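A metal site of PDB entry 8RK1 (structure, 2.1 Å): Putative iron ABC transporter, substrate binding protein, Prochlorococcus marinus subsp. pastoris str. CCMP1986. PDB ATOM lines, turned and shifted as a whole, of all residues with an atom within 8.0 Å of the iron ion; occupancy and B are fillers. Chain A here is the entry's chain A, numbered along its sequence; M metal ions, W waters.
The iron ion is bound by the side-chain hydroxyl (OH) of Tyr 200, at 1.9 Å.
The side-chain hydroxyl (OH) of Tyr 143 binds the iron ion.
The iron ion is bound by OH of Tyr 199 (2.0 Å).
OH of Tyr 13 is bound to the iron ion.
The iron ion is bound by water W1 (2.4 Å).
Within 4 Å of the iron ion: Tyr 13, Tyr 143, Tyr 199 and Tyr 200.
The nearest printed residue that does not touch the iron ion is Arg 103 (4.2 Å).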
ATOM      1  N   GLY A  10       0.652 -10.336  23.835  1.00  0.00           N
ATOM      2  CA  GLY A  10       0.411 -11.749  23.587  1.00  0.00           C
ATOM      3  C   GLY A  10       0.575 -12.637  24.822  1.00  0.00           C
ATOM      4  O   GLY A  10       0.349 -13.843  24.729  1.00  0.00           O
ATOM      5  N   HIS A  12      -0.873 -14.058  27.271  1.00  0.00           N
ATOM      6  CA  HIS A  12      -2.263 -14.333  27.541  1.00  0.00           C
ATOM      7  C   HIS A  12      -2.370 -15.280  28.740  1.00  0.00           C
ATOM      8  O   HIS A  12      -2.915 -16.372  28.618  1.00  0.00           O
ATOM      9  CB  HIS A  12      -2.844 -14.944  26.266  1.00  0.00           C
ATOM     10  CG  HIS A  12      -4.318 -14.868  26.136  1.00  0.00           C
ATOM     11  ND1 HIS A  12      -5.044 -15.527  25.159  1.00  0.00           N
ATOM     12  CD2 HIS A  12      -5.199 -14.200  26.900  1.00  0.00           C
ATOM     13  CE1 HIS A  12      -6.337 -15.247  25.339  1.00  0.00           C
ATOM     14  NE2 HIS A  12      -6.447 -14.441  26.380  1.00  0.00           N
ATOM     15  N   TYR A  13      -1.826 -14.870  29.890  1.00  0.00           N
ATOM     16  CA  TYR A  13      -1.848 -15.681  31.094  1.00  0.00           C
ATOM     17  C   TYR A  13      -2.818 -15.090  32.116  1.00  0.00           C
ATOM     18  O   TYR A  13      -3.159 -15.755  33.095  1.00  0.00           O
ATOM     19  CB  TYR A  13      -0.403 -15.750  31.581  1.00  0.00           C
ATOM     20  CG  TYR A  13       0.523 -16.565  30.680  1.00  0.00           C
ATOM     21  CD1 TYR A  13       0.288 -17.928  30.470  1.00  0.00           C
ATOM     22  CD2 TYR A  13       1.610 -15.984  30.023  1.00  0.00           C
ATOM     23  CE1 TYR A  13       1.101 -18.690  29.646  1.00  0.00           C
ATOM     24  CE2 TYR A  13       2.436 -16.745  29.204  1.00  0.00           C
ATOM     25  CZ  TYR A  13       2.186 -18.090  29.021  1.00  0.00           C
ATOM     26  OH  TYR A  13       3.008 -18.818  28.217  1.00  0.00           O
ATOM     27  N   VAL A  60       4.839 -13.983  22.656  1.00  0.00           N
ATOM     28  CA  VAL A  60       5.408 -15.178  23.245  1.00  0.00           C
ATOM     29  C   VAL A  60       5.977 -16.053  22.131  1.00  0.00           C
ATOM     30  O   VAL A  60       5.311 -16.247  21.124  1.00  0.00           O
ATOM     31  CB  VAL A  60       4.327 -15.921  24.047  1.00  0.00           C
ATOM     32  CG1 VAL A  60       4.816 -17.291  24.508  1.00  0.00           C
ATOM     33  CG2 VAL A  60       3.827 -15.063  25.202  1.00  0.00           C
ATOM     34  N   ASP A  61       7.216 -16.510  22.337  1.00  0.00           N
ATOM     35  CA  ASP A  61       7.883 -17.570  21.593  1.00  0.00           C
ATOM     36  C   ASP A  61       8.586 -17.015  20.354  1.00  0.00           C
ATOM     37  O   ASP A  61       8.053 -16.149  19.663  1.00  0.00           O
ATOM     38  CB  ASP A  61       6.962 -18.709  21.141  1.00  0.00           C
ATOM     39  CG  ASP A  61       7.720 -19.887  20.561  1.00  0.00           C
ATOM     40  OD1 ASP A  61       8.264 -19.759  19.440  1.00  0.00           O
ATOM     41  OD2 ASP A  61       7.773 -20.935  21.217  1.00  0.00           O
ATOM     42  N   ARG A 103      11.723 -19.203  29.324  1.00  0.00           N
ATOM     43  CA  ARG A 103      11.078 -20.468  29.621  1.00  0.00           C
ATOM     44  C   ARG A 103      11.899 -21.608  29.012  1.00  0.00           C
ATOM     45  O   ARG A 103      12.714 -21.404  28.114  1.00  0.00           O
ATOM     46  CB  ARG A 103       9.625 -20.488  29.133  1.00  0.00           C
ATOM     47  CG  ARG A 103       9.438 -20.201  27.650  1.00  0.00           C
ATOM     48  CD  ARG A 103       9.157 -18.735  27.303  1.00  0.00           C
ATOM     49  NE  ARG A 103       7.941 -18.199  27.899  1.00  0.00           N
ATOM     50  CZ  ARG A 103       6.710 -18.583  27.563  1.00  0.00           C
ATOM     51  NH1 ARG A 103       6.552 -19.331  26.473  1.00  0.00           N
ATOM     52  NH2 ARG A 103       5.687 -18.126  28.263  1.00  0.00           N
ATOM     53  N   ARG A 105      11.519 -25.569  27.462  1.00  0.00           N
ATOM     54  CA  ARG A 105      10.728 -26.722  27.076  1.00  0.00           C
ATOM     55  C   ARG A 105      11.488 -27.962  27.550  1.00  0.00           C
ATOM     56  O   ARG A 105      12.664 -28.102  27.253  1.00  0.00           O
ATOM     57  CB  ARG A 105      10.430 -26.723  25.573  1.00  0.00           C
ATOM     58  CG  ARG A 105       9.236 -27.593  25.199  1.00  0.00           C
ATOM     59  CD  ARG A 105       8.546 -27.084  23.954  1.00  0.00           C
ATOM     60  NE  ARG A 105       7.283 -27.789  23.693  1.00  0.00           N
ATOM     61  CZ  ARG A 105       6.151 -27.655  24.381  1.00  0.00           C
ATOM     62  NH1 ARG A 105       6.042 -26.776  25.376  1.00  0.00           N
ATOM     63  NH2 ARG A 105       5.083 -28.330  23.974  1.00  0.00           N
ATOM     64  N   ARG A 137       2.333 -32.738  22.392  1.00  0.00           N
ATOM     65  CA  ARG A 137       1.413 -31.753  21.872  1.00  0.00           C
ATOM     66  C   ARG A 137       1.608 -31.708  20.355  1.00  0.00           C
ATOM     67  O   ARG A 137       2.670 -32.066  19.848  1.00  0.00           O
ATOM     68  CB  ARG A 137       1.640 -30.412  22.575  1.00  0.00           C
ATOM     69  CG  ARG A 137       0.765 -29.281  22.062  1.00  0.00           C
ATOM     70  CD  ARG A 137       1.043 -28.002  22.847  1.00  0.00           C
ATOM     71  NE  ARG A 137       0.193 -26.875  22.472  1.00  0.00           N
ATOM     72  CZ  ARG A 137       0.033 -25.783  23.211  1.00  0.00           C
ATOM     73  NH1 ARG A 137       0.676 -25.631  24.354  1.00  0.00           N
ATOM     74  NH2 ARG A 137      -0.817 -24.845  22.813  1.00  0.00           N
ATOM     75  N   SER A 141       1.665 -25.973  17.797  1.00  0.00           N
ATOM     76  CA  SER A 141       2.224 -25.190  18.890  1.00  0.00           C
ATOM     77  C   SER A 141       3.536 -24.571  18.431  1.00  0.00           C
ATOM     78  O   SER A 141       4.430 -25.296  18.021  1.00  0.00           O
ATOM     79  CB  SER A 141       2.456 -26.030  20.116  1.00  0.00           C
ATOM     80  OG  SER A 141       2.779 -25.224  21.238  1.00  0.00           O
ATOM     81  N   TYR A 143       5.757 -23.595  20.341  1.00  0.00           N
ATOM     82  CA  TYR A 143       6.691 -24.158  21.310  1.00  0.00           C
ATOM     83  C   TYR A 143       7.427 -25.322  20.670  1.00  0.00           C
ATOM     84  O   TYR A 143       8.666 -25.367  20.703  1.00  0.00           O
ATOM     85  CB  TYR A 143       5.880 -24.623  22.529  1.00  0.00           C
ATOM     86  CG  TYR A 143       5.189 -23.521  23.332  1.00  0.00           C
ATOM     87  CD1 TYR A 143       5.537 -22.186  23.182  1.00  0.00           C
ATOM     88  CD2 TYR A 143       4.163 -23.835  24.214  1.00  0.00           C
ATOM     89  CE1 TYR A 143       4.904 -21.187  23.908  1.00  0.00           C
ATOM     90  CE2 TYR A 143       3.518 -22.855  24.939  1.00  0.00           C
ATOM     91  CZ  TYR A 143       3.883 -21.531  24.790  1.00  0.00           C
ATOM     92  OH  TYR A 143       3.252 -20.565  25.524  1.00  0.00           O
ATOM     93  N   ASP A 179      -0.403 -28.024  26.578  1.00  0.00           N
ATOM     94  CA  ASP A 179       0.630 -28.574  27.426  1.00  0.00           C
ATOM     95  C   ASP A 179       0.037 -29.078  28.731  1.00  0.00           C
ATOM     96  O   ASP A 179       0.467 -30.105  29.257  1.00  0.00           O
ATOM     97  CB  ASP A 179       1.692 -27.522  27.770  1.00  0.00           C
ATOM     98  CG  ASP A 179       2.799 -27.338  26.736  1.00  0.00           C
ATOM     99  OD1 ASP A 179       2.622 -27.804  25.590  1.00  0.00           O
ATOM    100  OD2 ASP A 179       3.838 -26.769  27.104  1.00  0.00           O
ATOM    101  N   SER A 180      -0.943 -28.331  29.238  1.00  0.00           N
ATOM    102  CA  SER A 180      -1.575 -28.581  30.525  1.00  0.00           C
ATOM    103  C   SER A 180      -2.224 -29.957  30.541  1.00  0.00           C
ATOM    104  O   SER A 180      -2.034 -30.703  31.481  1.00  0.00           O
ATOM    105  CB  SER A 180      -2.597 -27.529  30.813  1.00  0.00           C
ATOM    106  OG  SER A 180      -1.997 -26.240  30.900  1.00  0.00           O
ATOM    107  N   ASN A 197       6.432 -26.952  28.534  1.00  0.00           N
ATOM    108  CA  ASN A 197       7.140 -25.836  29.117  1.00  0.00           C
ATOM    109  C   ASN A 197       7.142 -25.981  30.648  1.00  0.00           C
ATOM    110  O   ASN A 197       6.154 -26.414  31.227  1.00  0.00           O
ATOM    111  CB  ASN A 197       6.511 -24.518  28.673  1.00  0.00           C
ATOM    112  CG  ASN A 197       6.888 -24.120  27.257  1.00  0.00           C
ATOM    113  OD1 ASN A 197       7.778 -24.721  26.659  1.00  0.00           O
ATOM    114  ND2 ASN A 197       6.285 -23.048  26.735  1.00  0.00           N
ATOM    115  N   TYR A 199       6.982 -23.932  33.157  1.00  0.00           N
ATOM    116  CA  TYR A 199       6.129 -23.082  33.986  1.00  0.00           C
ATOM    117  C   TYR A 199       4.721 -23.638  34.169  1.00  0.00           C
ATOM    118  O   TYR A 199       4.106 -23.383  35.194  1.00  0.00           O
ATOM    119  CB  TYR A 199       6.068 -21.641  33.475  1.00  0.00           C
ATOM    120  CG  TYR A 199       5.597 -21.424  32.038  1.00  0.00           C
ATOM    121  CD1 TYR A 199       4.259 -21.321  31.702  1.00  0.00           C
ATOM    122  CD2 TYR A 199       6.523 -21.318  31.015  1.00  0.00           C
ATOM    123  CE1 TYR A 199       3.853 -21.137  30.391  1.00  0.00           C
ATOM    124  CE2 TYR A 199       6.137 -21.141  29.697  1.00  0.00           C
ATOM    125  CZ  TYR A 199       4.802 -21.052  29.378  1.00  0.00           C
ATOM    126  OH  TYR A 199       4.449 -20.876  28.072  1.00  0.00           O
ATOM    127  N   TYR A 200       4.221 -24.442  33.229  1.00  0.00           N
ATOM    128  CA  TYR A 200       2.926 -25.102  33.368  1.00  0.00           C
ATOM    129  C   TYR A 200       2.963 -26.147  34.490  1.00  0.00           C
ATOM    130  O   TYR A 200       1.957 -26.337  35.182  1.00  0.00           O
ATOM    131  CB  TYR A 200       2.498 -25.792  32.076  1.00  0.00           C
ATOM    132  CG  TYR A 200       2.212 -24.842  30.930  1.00  0.00           C
ATOM    133  CD1 TYR A 200       1.243 -23.853  31.054  1.00  0.00           C
ATOM    134  CD2 TYR A 200       2.894 -24.934  29.717  1.00  0.00           C
ATOM    135  CE1 TYR A 200       0.965 -22.973  30.019  1.00  0.00           C
ATOM    136  CE2 TYR A 200       2.604 -24.076  28.666  1.00  0.00           C
ATOM    137  CZ  TYR A 200       1.650 -23.096  28.827  1.00  0.00           C
ATOM    138  OH  TYR A 200       1.387 -22.231  27.801  1.00  0.00           O
ATOM    139  N   ARG A 203       2.936 -24.002  37.744  1.00  0.00           N
ATOM    140  CA  ARG A 203       1.640 -23.367  37.982  1.00  0.00           C
ATOM    141  C   ARG A 203       0.625 -24.346  38.563  1.00  0.00           C
ATOM    142  O   ARG A 203      -0.176 -23.991  39.414  1.00  0.00           O
ATOM    143  CB  ARG A 203       1.070 -22.785  36.688  1.00  0.00           C
ATOM    144  CG  ARG A 203       1.882 -21.616  36.160  1.00  0.00           C
ATOM    145  CD  ARG A 203       1.393 -21.213  34.785  1.00  0.00           C
ATOM    146  NE  ARG A 203       0.289 -20.286  34.933  1.00  0.00           N
ATOM    147  CZ  ARG A 203      -0.849 -20.314  34.255  1.00  0.00           C
ATOM    148  NH1 ARG A 203      -1.193 -21.374  33.541  1.00  0.00           N
ATOM    149  NH2 ARG A 203      -1.647 -19.264  34.343  1.00  0.00           N
ATOM    150  N   THR A 233       9.630 -14.725  25.969  1.00  0.00           N
ATOM    151  CA  THR A 233       8.693 -13.678  25.604  1.00  0.00           C
ATOM    152  C   THR A 233       9.507 -12.402  25.364  1.00  0.00           C
ATOM    153  O   THR A 233      10.580 -12.226  25.927  1.00  0.00           O
ATOM    154  CB  THR A 233       7.570 -13.513  26.640  1.00  0.00           C
ATOM    155  OG1 THR A 233       8.153 -12.839  27.770  1.00  0.00           O
ATOM    156  CG2 THR A 233       7.008 -14.837  27.103  1.00  0.00           C
ATOM    157  N   THR A 267       4.163 -15.720  36.075  1.00  0.00           N
ATOM    158  CA  THR A 267       3.927 -16.883  35.246  1.00  0.00           C
ATOM    159  C   THR A 267       4.866 -18.041  35.592  1.00  0.00           C
ATOM    160  O   THR A 267       4.871 -19.038  34.865  1.00  0.00           O
ATOM    161  CB  THR A 267       4.090 -16.493  33.769  1.00  0.00           C
ATOM    162  OG1 THR A 267       5.259 -15.689  33.666  1.00  0.00           O
ATOM    163  CG2 THR A 267       2.901 -15.709  33.237  1.00  0.00           C
ATOM    164  N   GLU A 269       8.001 -18.106  35.271  1.00  0.00           N
ATOM    165  CA  GLU A 269       9.128 -18.160  34.362  1.00  0.00           C
ATOM    166  C   GLU A 269      10.391 -17.726  35.077  1.00  0.00           C
ATOM    167  O   GLU A 269      10.366 -17.386  36.260  1.00  0.00           O
ATOM    168  CB  GLU A 269       8.878 -17.272  33.141  1.00  0.00           C
ATOM    169  CG  GLU A 269       7.765 -17.786  32.242  1.00  0.00           C
ATOM    170  CD  GLU A 269       7.470 -16.772  31.149  1.00  0.00           C
ATOM    171  OE1 GLU A 269       6.533 -15.989  31.324  1.00  0.00           O
ATOM    172  OE2 GLU A 269       8.216 -16.762  30.140  1.00  0.00           O
HETATM  173 FE    FE M   1       2.585 -20.782  27.345  1.00  0.00          FE
HETATM  174  O   HOH W   1       0.754 -19.483  26.566  1.00  0.00           O
